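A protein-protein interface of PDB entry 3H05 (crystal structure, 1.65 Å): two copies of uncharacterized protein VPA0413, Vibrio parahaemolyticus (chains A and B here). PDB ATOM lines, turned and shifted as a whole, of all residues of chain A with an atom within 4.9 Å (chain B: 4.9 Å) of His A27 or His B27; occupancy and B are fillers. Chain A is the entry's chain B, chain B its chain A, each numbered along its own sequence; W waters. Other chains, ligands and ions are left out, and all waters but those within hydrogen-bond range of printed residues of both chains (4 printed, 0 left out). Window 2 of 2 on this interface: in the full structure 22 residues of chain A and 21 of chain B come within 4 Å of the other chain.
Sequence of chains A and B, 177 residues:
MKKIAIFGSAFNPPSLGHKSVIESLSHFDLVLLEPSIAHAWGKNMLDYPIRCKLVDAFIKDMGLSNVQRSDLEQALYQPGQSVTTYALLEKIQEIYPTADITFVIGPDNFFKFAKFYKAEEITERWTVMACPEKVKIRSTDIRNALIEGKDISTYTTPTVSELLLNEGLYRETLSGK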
ATOM      1  N   LYS A   3      -1.223 -14.684  -6.337  1.00  0.00           N
ATOM      2  CA  LYS A   3      -1.866 -15.694  -7.201  1.00  0.00           C
ATOM      3  C   LYS A   3      -2.733 -15.024  -8.258  1.00  0.00           C
ATOM      4  O   LYS A   3      -3.756 -14.400  -7.938  1.00  0.00           O
ATOM      5  CB  LYS A   3      -2.748 -16.667  -6.385  1.00  0.00           C
ATOM      6  CG  LYS A   3      -2.010 -17.459  -5.296  1.00  0.00           C
ATOM      7  CD  LYS A   3      -0.896 -18.301  -5.871  1.00  0.00           C
ATOM      8  CE  LYS A   3      -0.225 -19.162  -4.799  1.00  0.00           C
ATOM      9  NZ  LYS A   3       0.814 -20.030  -5.400  1.00  0.00           N
ATOM     10  N   SER A  24     -15.647 -19.178 -10.156  1.00  0.00           N
ATOM     11  CA  SER A  24     -14.981 -20.247  -9.397  1.00  0.00           C
ATOM     12  C   SER A  24     -13.591 -19.870  -8.913  1.00  0.00           C
ATOM     13  O   SER A  24     -12.972 -20.654  -8.241  1.00  0.00           O
ATOM     14  CB  SER A  24     -14.887 -21.556 -10.207  1.00  0.00           C
ATOM     15  OG  SER A  24     -13.754 -21.530 -11.085  1.00  0.00           O
ATOM     16  N   LEU A  25     -13.131 -18.650  -9.218  1.00  0.00           N
ATOM     17  CA  LEU A  25     -11.732 -18.246  -9.027  1.00  0.00           C
ATOM     18  C   LEU A  25     -11.572 -17.258  -7.866  1.00  0.00           C
ATOM     19  O   LEU A  25     -10.619 -16.478  -7.834  1.00  0.00           O
ATOM     20  CB  LEU A  25     -11.193 -17.619 -10.330  1.00  0.00           C
ATOM     21  CG  LEU A  25     -11.312 -18.531 -11.559  1.00  0.00           C
ATOM     22  CD1 LEU A  25     -10.828 -17.777 -12.809  1.00  0.00           C
ATOM     23  CD2 LEU A  25     -10.525 -19.826 -11.373  1.00  0.00           C
ATOM     24  N   SER A  26     -12.482 -17.320  -6.897  1.00  0.00           N
ATOM     25  CA  SER A  26     -12.482 -16.357  -5.782  1.00  0.00           C
ATOM     26  C   SER A  26     -11.187 -16.447  -4.956  1.00  0.00           C
ATOM     27  O   SER A  26     -10.822 -15.487  -4.241  1.00  0.00           O
ATOM     28  CB  SER A  26     -13.709 -16.570  -4.888  1.00  0.00           C
ATOM     29  OG  SER A  26     -13.725 -17.885  -4.350  1.00  0.00           O
ATOM     30  N   HIS A  27     -10.509 -17.594  -5.040  1.00  0.00           N
ATOM     31  CA  HIS A  27      -9.295 -17.844  -4.247  1.00  0.00           C
ATOM     32  C   HIS A  27      -8.033 -17.255  -4.848  1.00  0.00           C
ATOM     33  O   HIS A  27      -6.981 -17.276  -4.221  1.00  0.00           O
ATOM     34  CB  HIS A  27      -9.101 -19.343  -3.912  1.00  0.00           C
ATOM     35  CG  HIS A  27      -9.209 -20.278  -5.077  1.00  0.00           C
ATOM     36  ND1 HIS A  27     -10.186 -20.173  -6.047  1.00  0.00           N
ATOM     37  CD2 HIS A  27      -8.497 -21.392  -5.378  1.00  0.00           C
ATOM     38  CE1 HIS A  27     -10.072 -21.184  -6.891  1.00  0.00           C
ATOM     39  NE2 HIS A  27      -9.046 -21.927  -6.523  1.00  0.00           N
ATOM     40  N   PHE A  28      -8.153 -16.719  -6.055  1.00  0.00           N
ATOM     41  CA  PHE A  28      -7.045 -15.980  -6.651  1.00  0.00           C
ATOM     42  C   PHE A  28      -7.085 -14.530  -6.223  1.00  0.00           C
ATOM     43  O   PHE A  28      -8.161 -13.974  -5.974  1.00  0.00           O
ATOM     44  CB  PHE A  28      -7.096 -16.111  -8.179  1.00  0.00           C
ATOM     45  CG  PHE A  28      -6.696 -17.465  -8.633  1.00  0.00           C
ATOM     46  CD1 PHE A  28      -5.361 -17.741  -8.940  1.00  0.00           C
ATOM     47  CD2 PHE A  28      -7.630 -18.501  -8.671  1.00  0.00           C
ATOM     48  CE1 PHE A  28      -4.960 -19.055  -9.307  1.00  0.00           C
ATOM     49  CE2 PHE A  28      -7.241 -19.792  -9.043  1.00  0.00           C
ATOM     50  CZ  PHE A  28      -5.915 -20.073  -9.361  1.00  0.00           C
ATOM     51  N   ASP A  29      -5.913 -13.914  -6.123  1.00  0.00           N
ATOM     52  CA  ASP A  29      -5.832 -12.502  -5.768  1.00  0.00           C
ATOM     53  C   ASP A  29      -6.289 -11.586  -6.899  1.00  0.00           C
ATOM     54  O   ASP A  29      -6.856 -10.514  -6.663  1.00  0.00           O
ATOM     55  CB  ASP A  29      -4.411 -12.164  -5.342  1.00  0.00           C
ATOM     56  CG  ASP A  29      -3.976 -12.947  -4.125  1.00  0.00           C
ATOM     57  OD1 ASP A  29      -4.648 -12.863  -3.068  1.00  0.00           O
ATOM     58  OD2 ASP A  29      -2.976 -13.675  -4.214  1.00  0.00           O
ATOM     59  N   ASN A  66     -12.246  -9.495  -7.553  1.00  0.00           N
ATOM     60  CA  ASN A  66     -10.894  -9.807  -8.023  1.00  0.00           C
ATOM     61  C   ASN A  66     -10.694  -9.819  -9.542  1.00  0.00           C
ATOM     62  O   ASN A  66      -9.604 -10.156  -9.999  1.00  0.00           O
ATOM     63  CB  ASN A  66     -10.350 -11.125  -7.398  1.00  0.00           C
ATOM     64  CG  ASN A  66     -11.047 -12.392  -7.950  1.00  0.00           C
ATOM     65  OD1 ASN A  66     -11.976 -12.309  -8.741  1.00  0.00           O
ATOM     66  ND2 ASN A  66     -10.600 -13.555  -7.496  1.00  0.00           N
ATOM     67  N   MET A 129      -5.416 -24.837 -15.452  1.00  0.00           N
ATOM     68  CA  MET A 129      -6.598 -25.207 -14.642  1.00  0.00           C
ATOM     69  C   MET A 129      -7.769 -25.279 -15.588  1.00  0.00           C
ATOM     70  O   MET A 129      -8.055 -24.304 -16.283  1.00  0.00           O
ATOM     71  CB  MET A 129      -6.841 -24.080 -13.598  1.00  0.00           C
ATOM     72  CG  MET A 129      -8.102 -24.182 -12.721  1.00  0.00           C
ATOM     73  SD  MET A 129      -8.160 -22.850 -11.440  1.00  0.00           S
ATOM     74  CE  MET A 129      -6.936 -23.508 -10.330  1.00  0.00           C
ATOM     75  N   LYS B   3     -12.472 -23.986  -0.677  1.00  0.00           N
ATOM     76  CA  LYS B   3     -11.681 -24.477  -1.812  1.00  0.00           C
ATOM     77  C   LYS B   3     -10.778 -25.617  -1.362  1.00  0.00           C
ATOM     78  O   LYS B   3      -9.850 -25.416  -0.553  1.00  0.00           O
ATOM     79  CB  LYS B   3     -10.831 -23.355  -2.409  1.00  0.00           C
ATOM     80  CG  LYS B   3     -11.651 -22.193  -2.992  1.00  0.00           C
ATOM     81  CD  LYS B   3     -12.505 -22.615  -4.181  1.00  0.00           C
ATOM     82  CE  LYS B   3     -13.213 -21.393  -4.816  1.00  0.00           C
ATOM     83  NZ  LYS B   3     -14.231 -21.818  -5.815  1.00  0.00           N
ATOM     84  N   SER B  24       2.658 -24.855  -4.067  1.00  0.00           N
ATOM     85  CA  SER B  24       2.036 -23.867  -4.950  1.00  0.00           C
ATOM     86  C   SER B  24       0.570 -23.623  -4.606  1.00  0.00           C
ATOM     87  O   SER B  24      -0.073 -22.788  -5.238  1.00  0.00           O
ATOM     88  CB  SER B  24       2.146 -24.261  -6.430  1.00  0.00           C
ATOM     89  OG  SER B  24       1.146 -25.209  -6.798  1.00  0.00           O
ATOM     90  N   LEU B  25       0.063 -24.336  -3.599  1.00  0.00           N
ATOM     91  CA  LEU B  25      -1.396 -24.404  -3.353  1.00  0.00           C
ATOM     92  C   LEU B  25      -1.851 -23.652  -2.100  1.00  0.00           C
ATOM     93  O   LEU B  25      -2.872 -23.987  -1.480  1.00  0.00           O
ATOM     94  CB  LEU B  25      -1.869 -25.863  -3.321  1.00  0.00           C
ATOM     95  CG  LEU B  25      -1.525 -26.719  -4.534  1.00  0.00           C
ATOM     96  CD1 LEU B  25      -1.947 -28.189  -4.336  1.00  0.00           C
ATOM     97  CD2 LEU B  25      -2.191 -26.154  -5.774  1.00  0.00           C
ATOM     98  N   SER B  26      -1.115 -22.606  -1.751  1.00  0.00           N
ATOM     99  CA  SER B  26      -1.400 -21.837  -0.542  1.00  0.00           C
ATOM    100  C   SER B  26      -2.753 -21.117  -0.565  1.00  0.00           C
ATOM    101  O   SER B  26      -3.279 -20.754   0.506  1.00  0.00           O
ATOM    102  CB  SER B  26      -0.283 -20.818  -0.294  1.00  0.00           C
ATOM    103  OG  SER B  26      -0.294 -19.825  -1.318  1.00  0.00           O
ATOM    104  N   HIS B  27      -3.291 -20.890  -1.770  1.00  0.00           N
ATOM    105  CA  HIS B  27      -4.584 -20.232  -1.945  1.00  0.00           C
ATOM    106  C   HIS B  27      -5.773 -21.187  -1.738  1.00  0.00           C
ATOM    107  O   HIS B  27      -6.920 -20.747  -1.728  1.00  0.00           O
ATOM    108  CB  HIS B  27      -4.686 -19.532  -3.329  1.00  0.00           C
ATOM    109  CG  HIS B  27      -4.175 -20.359  -4.469  1.00  0.00           C
ATOM    110  ND1 HIS B  27      -4.774 -20.376  -5.717  1.00  0.00           N
ATOM    111  CD2 HIS B  27      -3.106 -21.185  -4.550  1.00  0.00           C
ATOM    112  CE1 HIS B  27      -4.078 -21.176  -6.515  1.00  0.00           C
ATOM    113  NE2 HIS B  27      -3.066 -21.677  -5.828  1.00  0.00           N
ATOM    114  N   PHE B  28      -5.502 -22.487  -1.574  1.00  0.00           N
ATOM    115  CA  PHE B  28      -6.571 -23.425  -1.199  1.00  0.00           C
ATOM    116  C   PHE B  28      -6.761 -23.479   0.304  1.00  0.00           C
ATOM    117  O   PHE B  28      -5.814 -23.265   1.079  1.00  0.00           O
ATOM    118  CB  PHE B  28      -6.302 -24.818  -1.773  1.00  0.00           C
ATOM    119  CG  PHE B  28      -6.529 -24.863  -3.248  1.00  0.00           C
ATOM    120  CD1 PHE B  28      -7.762 -25.256  -3.766  1.00  0.00           C
ATOM    121  CD2 PHE B  28      -5.527 -24.433  -4.125  1.00  0.00           C
ATOM    122  CE1 PHE B  28      -8.015 -25.246  -5.141  1.00  0.00           C
ATOM    123  CE2 PHE B  28      -5.753 -24.418  -5.497  1.00  0.00           C
ATOM    124  CZ  PHE B  28      -7.004 -24.840  -6.022  1.00  0.00           C
ATOM    125  N   ASP B  29      -8.007 -23.703   0.728  1.00  0.00           N
ATOM    126  CA  ASP B  29      -8.301 -23.780   2.165  1.00  0.00           C
ATOM    127  C   ASP B  29      -7.797 -25.071   2.763  1.00  0.00           C
ATOM    128  O   ASP B  29      -7.384 -25.105   3.935  1.00  0.00           O
ATOM    129  CB  ASP B  29      -9.801 -23.638   2.413  1.00  0.00           C
ATOM    130  CG  ASP B  29     -10.322 -22.298   1.955  1.00  0.00           C
ATOM    131  OD1 ASP B  29      -9.691 -21.261   2.305  1.00  0.00           O
ATOM    132  OD2 ASP B  29     -11.361 -22.269   1.260  1.00  0.00           O
ATOM    133  N   ASN B  66      -2.158 -25.728   5.437  1.00  0.00           N
ATOM    134  CA  ASN B  66      -3.362 -26.226   4.759  1.00  0.00           C
ATOM    135  C   ASN B  66      -3.325 -27.680   4.293  1.00  0.00           C
ATOM    136  O   ASN B  66      -4.280 -28.149   3.681  1.00  0.00           O
ATOM    137  CB  ASN B  66      -3.797 -25.282   3.614  1.00  0.00           C
ATOM    138  CG  ASN B  66      -2.859 -25.326   2.424  1.00  0.00           C
ATOM    139  OD1 ASN B  66      -1.827 -25.960   2.473  1.00  0.00           O
ATOM    140  ND2 ASN B  66      -3.214 -24.609   1.353  1.00  0.00           N
HETATM  141  O   HOH W   1       1.682 -21.151  -2.906  1.00  0.00           O
HETATM  142  O   HOH W   2       0.129 -21.091  -8.116  1.00  0.00           O
HETATM  143  O   HOH W   3     -15.216 -19.130  -6.231  1.00  0.00           O
HETATM  144  O   HOH W   4     -12.967 -24.018  -7.458  1.00  0.00           O
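The backbone carbonyl oxygen (O) of Ser A24 is in hydrogen-bond range of the side-chain amino group (NZ) of Lys B3. NZ of Lys A3 is in hydrogen-bond range of O of Ser B24.
The backbone NH of Lys B3 is in hydrogen-bond range of the side-chain carboxylate of Asp B29. The backbone carbonyl oxygen (O) of Ser B24 sits at hydrogen-bond distance from a ring nitrogen (NE2) of His B27. O of Phe B28 is in hydrogen-bond range of ND2 of Asn B66, at 2.9 Å. O of Lys A3 sits at hydrogen-bond distance from N of Asp A29 (2.9 Å). The backbone carbonyl oxygen (O) of Phe A28 sits at hydrogen-bond distance from the side-chain amide nitrogen (ND2) of Asn A66 (2.9 Å).
CE of Lys A3 touches OG of Ser B26 (3.5 Å). His B27 touches Lys A3 (CD2 to CE, 3.5 Å). Lys B3 touches Ser A26 (CE to OG, 3.6 Å). CE of Lys B3 touches ND1 of His A27 (3.5 Å). His A27 touches His B27 (O to CB, 3.3 Å). NE2 of His A27 touches CZ of Phe B28, at 3.6 Å. His B27 touches Phe A28 (CE1 to CZ, 3.6 Å).
Printed residues of chain B within 4 Å of His A27: Lys B3 (3.5 Å), His B27 (3.3 Å) and Phe B28 (3.6 Å). Of the printed residues of chain A, Lys B3 touches Ser A24, Ser A26 and His A27. Leu B25 touches none of the printed residues of chain A. Of chain A, only Lys A3 (3.5 Å), His A27 (3.3 Å) and Phe A28 (3.6 Å) come within 4 Å of His B27. Of the printed residues of chain A, Phe B28 touches His A27 (3.6 Å). The nearest printed residue of chain B that does not touch His A27 is Asp B29 (6.4 Å). The nearest printed residue of chain B that does not touch Phe A28 is Phe B28 (5.8 Å).
Of the 8 printed residues of chain B, 5 touch a printed residue of chain A. Hydrophobic or aromatic side chains of chain B within 4 Å of the printed part of chain A: His B27 and Phe B28. Of the 9 printed residues of chain A, 5 touch a printed residue of chain B. Along chain A the printed residues that touch a printed residue of chain B span positions 3 to 28. Among the printed residues, 9 pairs touch across the chains. Among the printed residues, no Asp or Glu carboxylate lies within 4 Å of a Lys or Arg side-chain nitrogen of the other chain.
Lys A3 touches Ser B24, and with the chains exchanged Ser A24 touches Lys B3. Lys A3 touches Ser B26, and with the chains exchanged Ser A26 touches Lys B3. Lys A3 touches His B27, and with the chains exchanged His A27 touches Lys B3. His A27 touches Phe B28, and with the chains exchanged Phe A28 touches His B27. Of the 9 pairs that touch across the chains among the printed residues, 9 have their exchanged pair printed and touching as well.
Water W3 lies within hydrogen-bond range of OG of Ser A26 (2.7 Å), NZ of Lys B3 (2.9 Å) and O of Ser A24 (3.4 Å). Water W1 lies within hydrogen-bond range of the side-chain hydroxyl (OG) of Ser B26 (2.9 Å), the side-chain amino group (NZ) of Lys A3 (2.9 Å) and the backbone carbonyl oxygen (O) of Ser B24 (3.3 Å). Water W2 bridges the side-chain amino group of Lys A3 (3.0 Å) and the backbone carbonyl oxygen of Ser B24 (3.3 Å). Water W4 bridges the side-chain amino group of Lys B3 (3.0 Å) and the backbone carbonyl oxygen of Ser A24 (3.5 Å).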
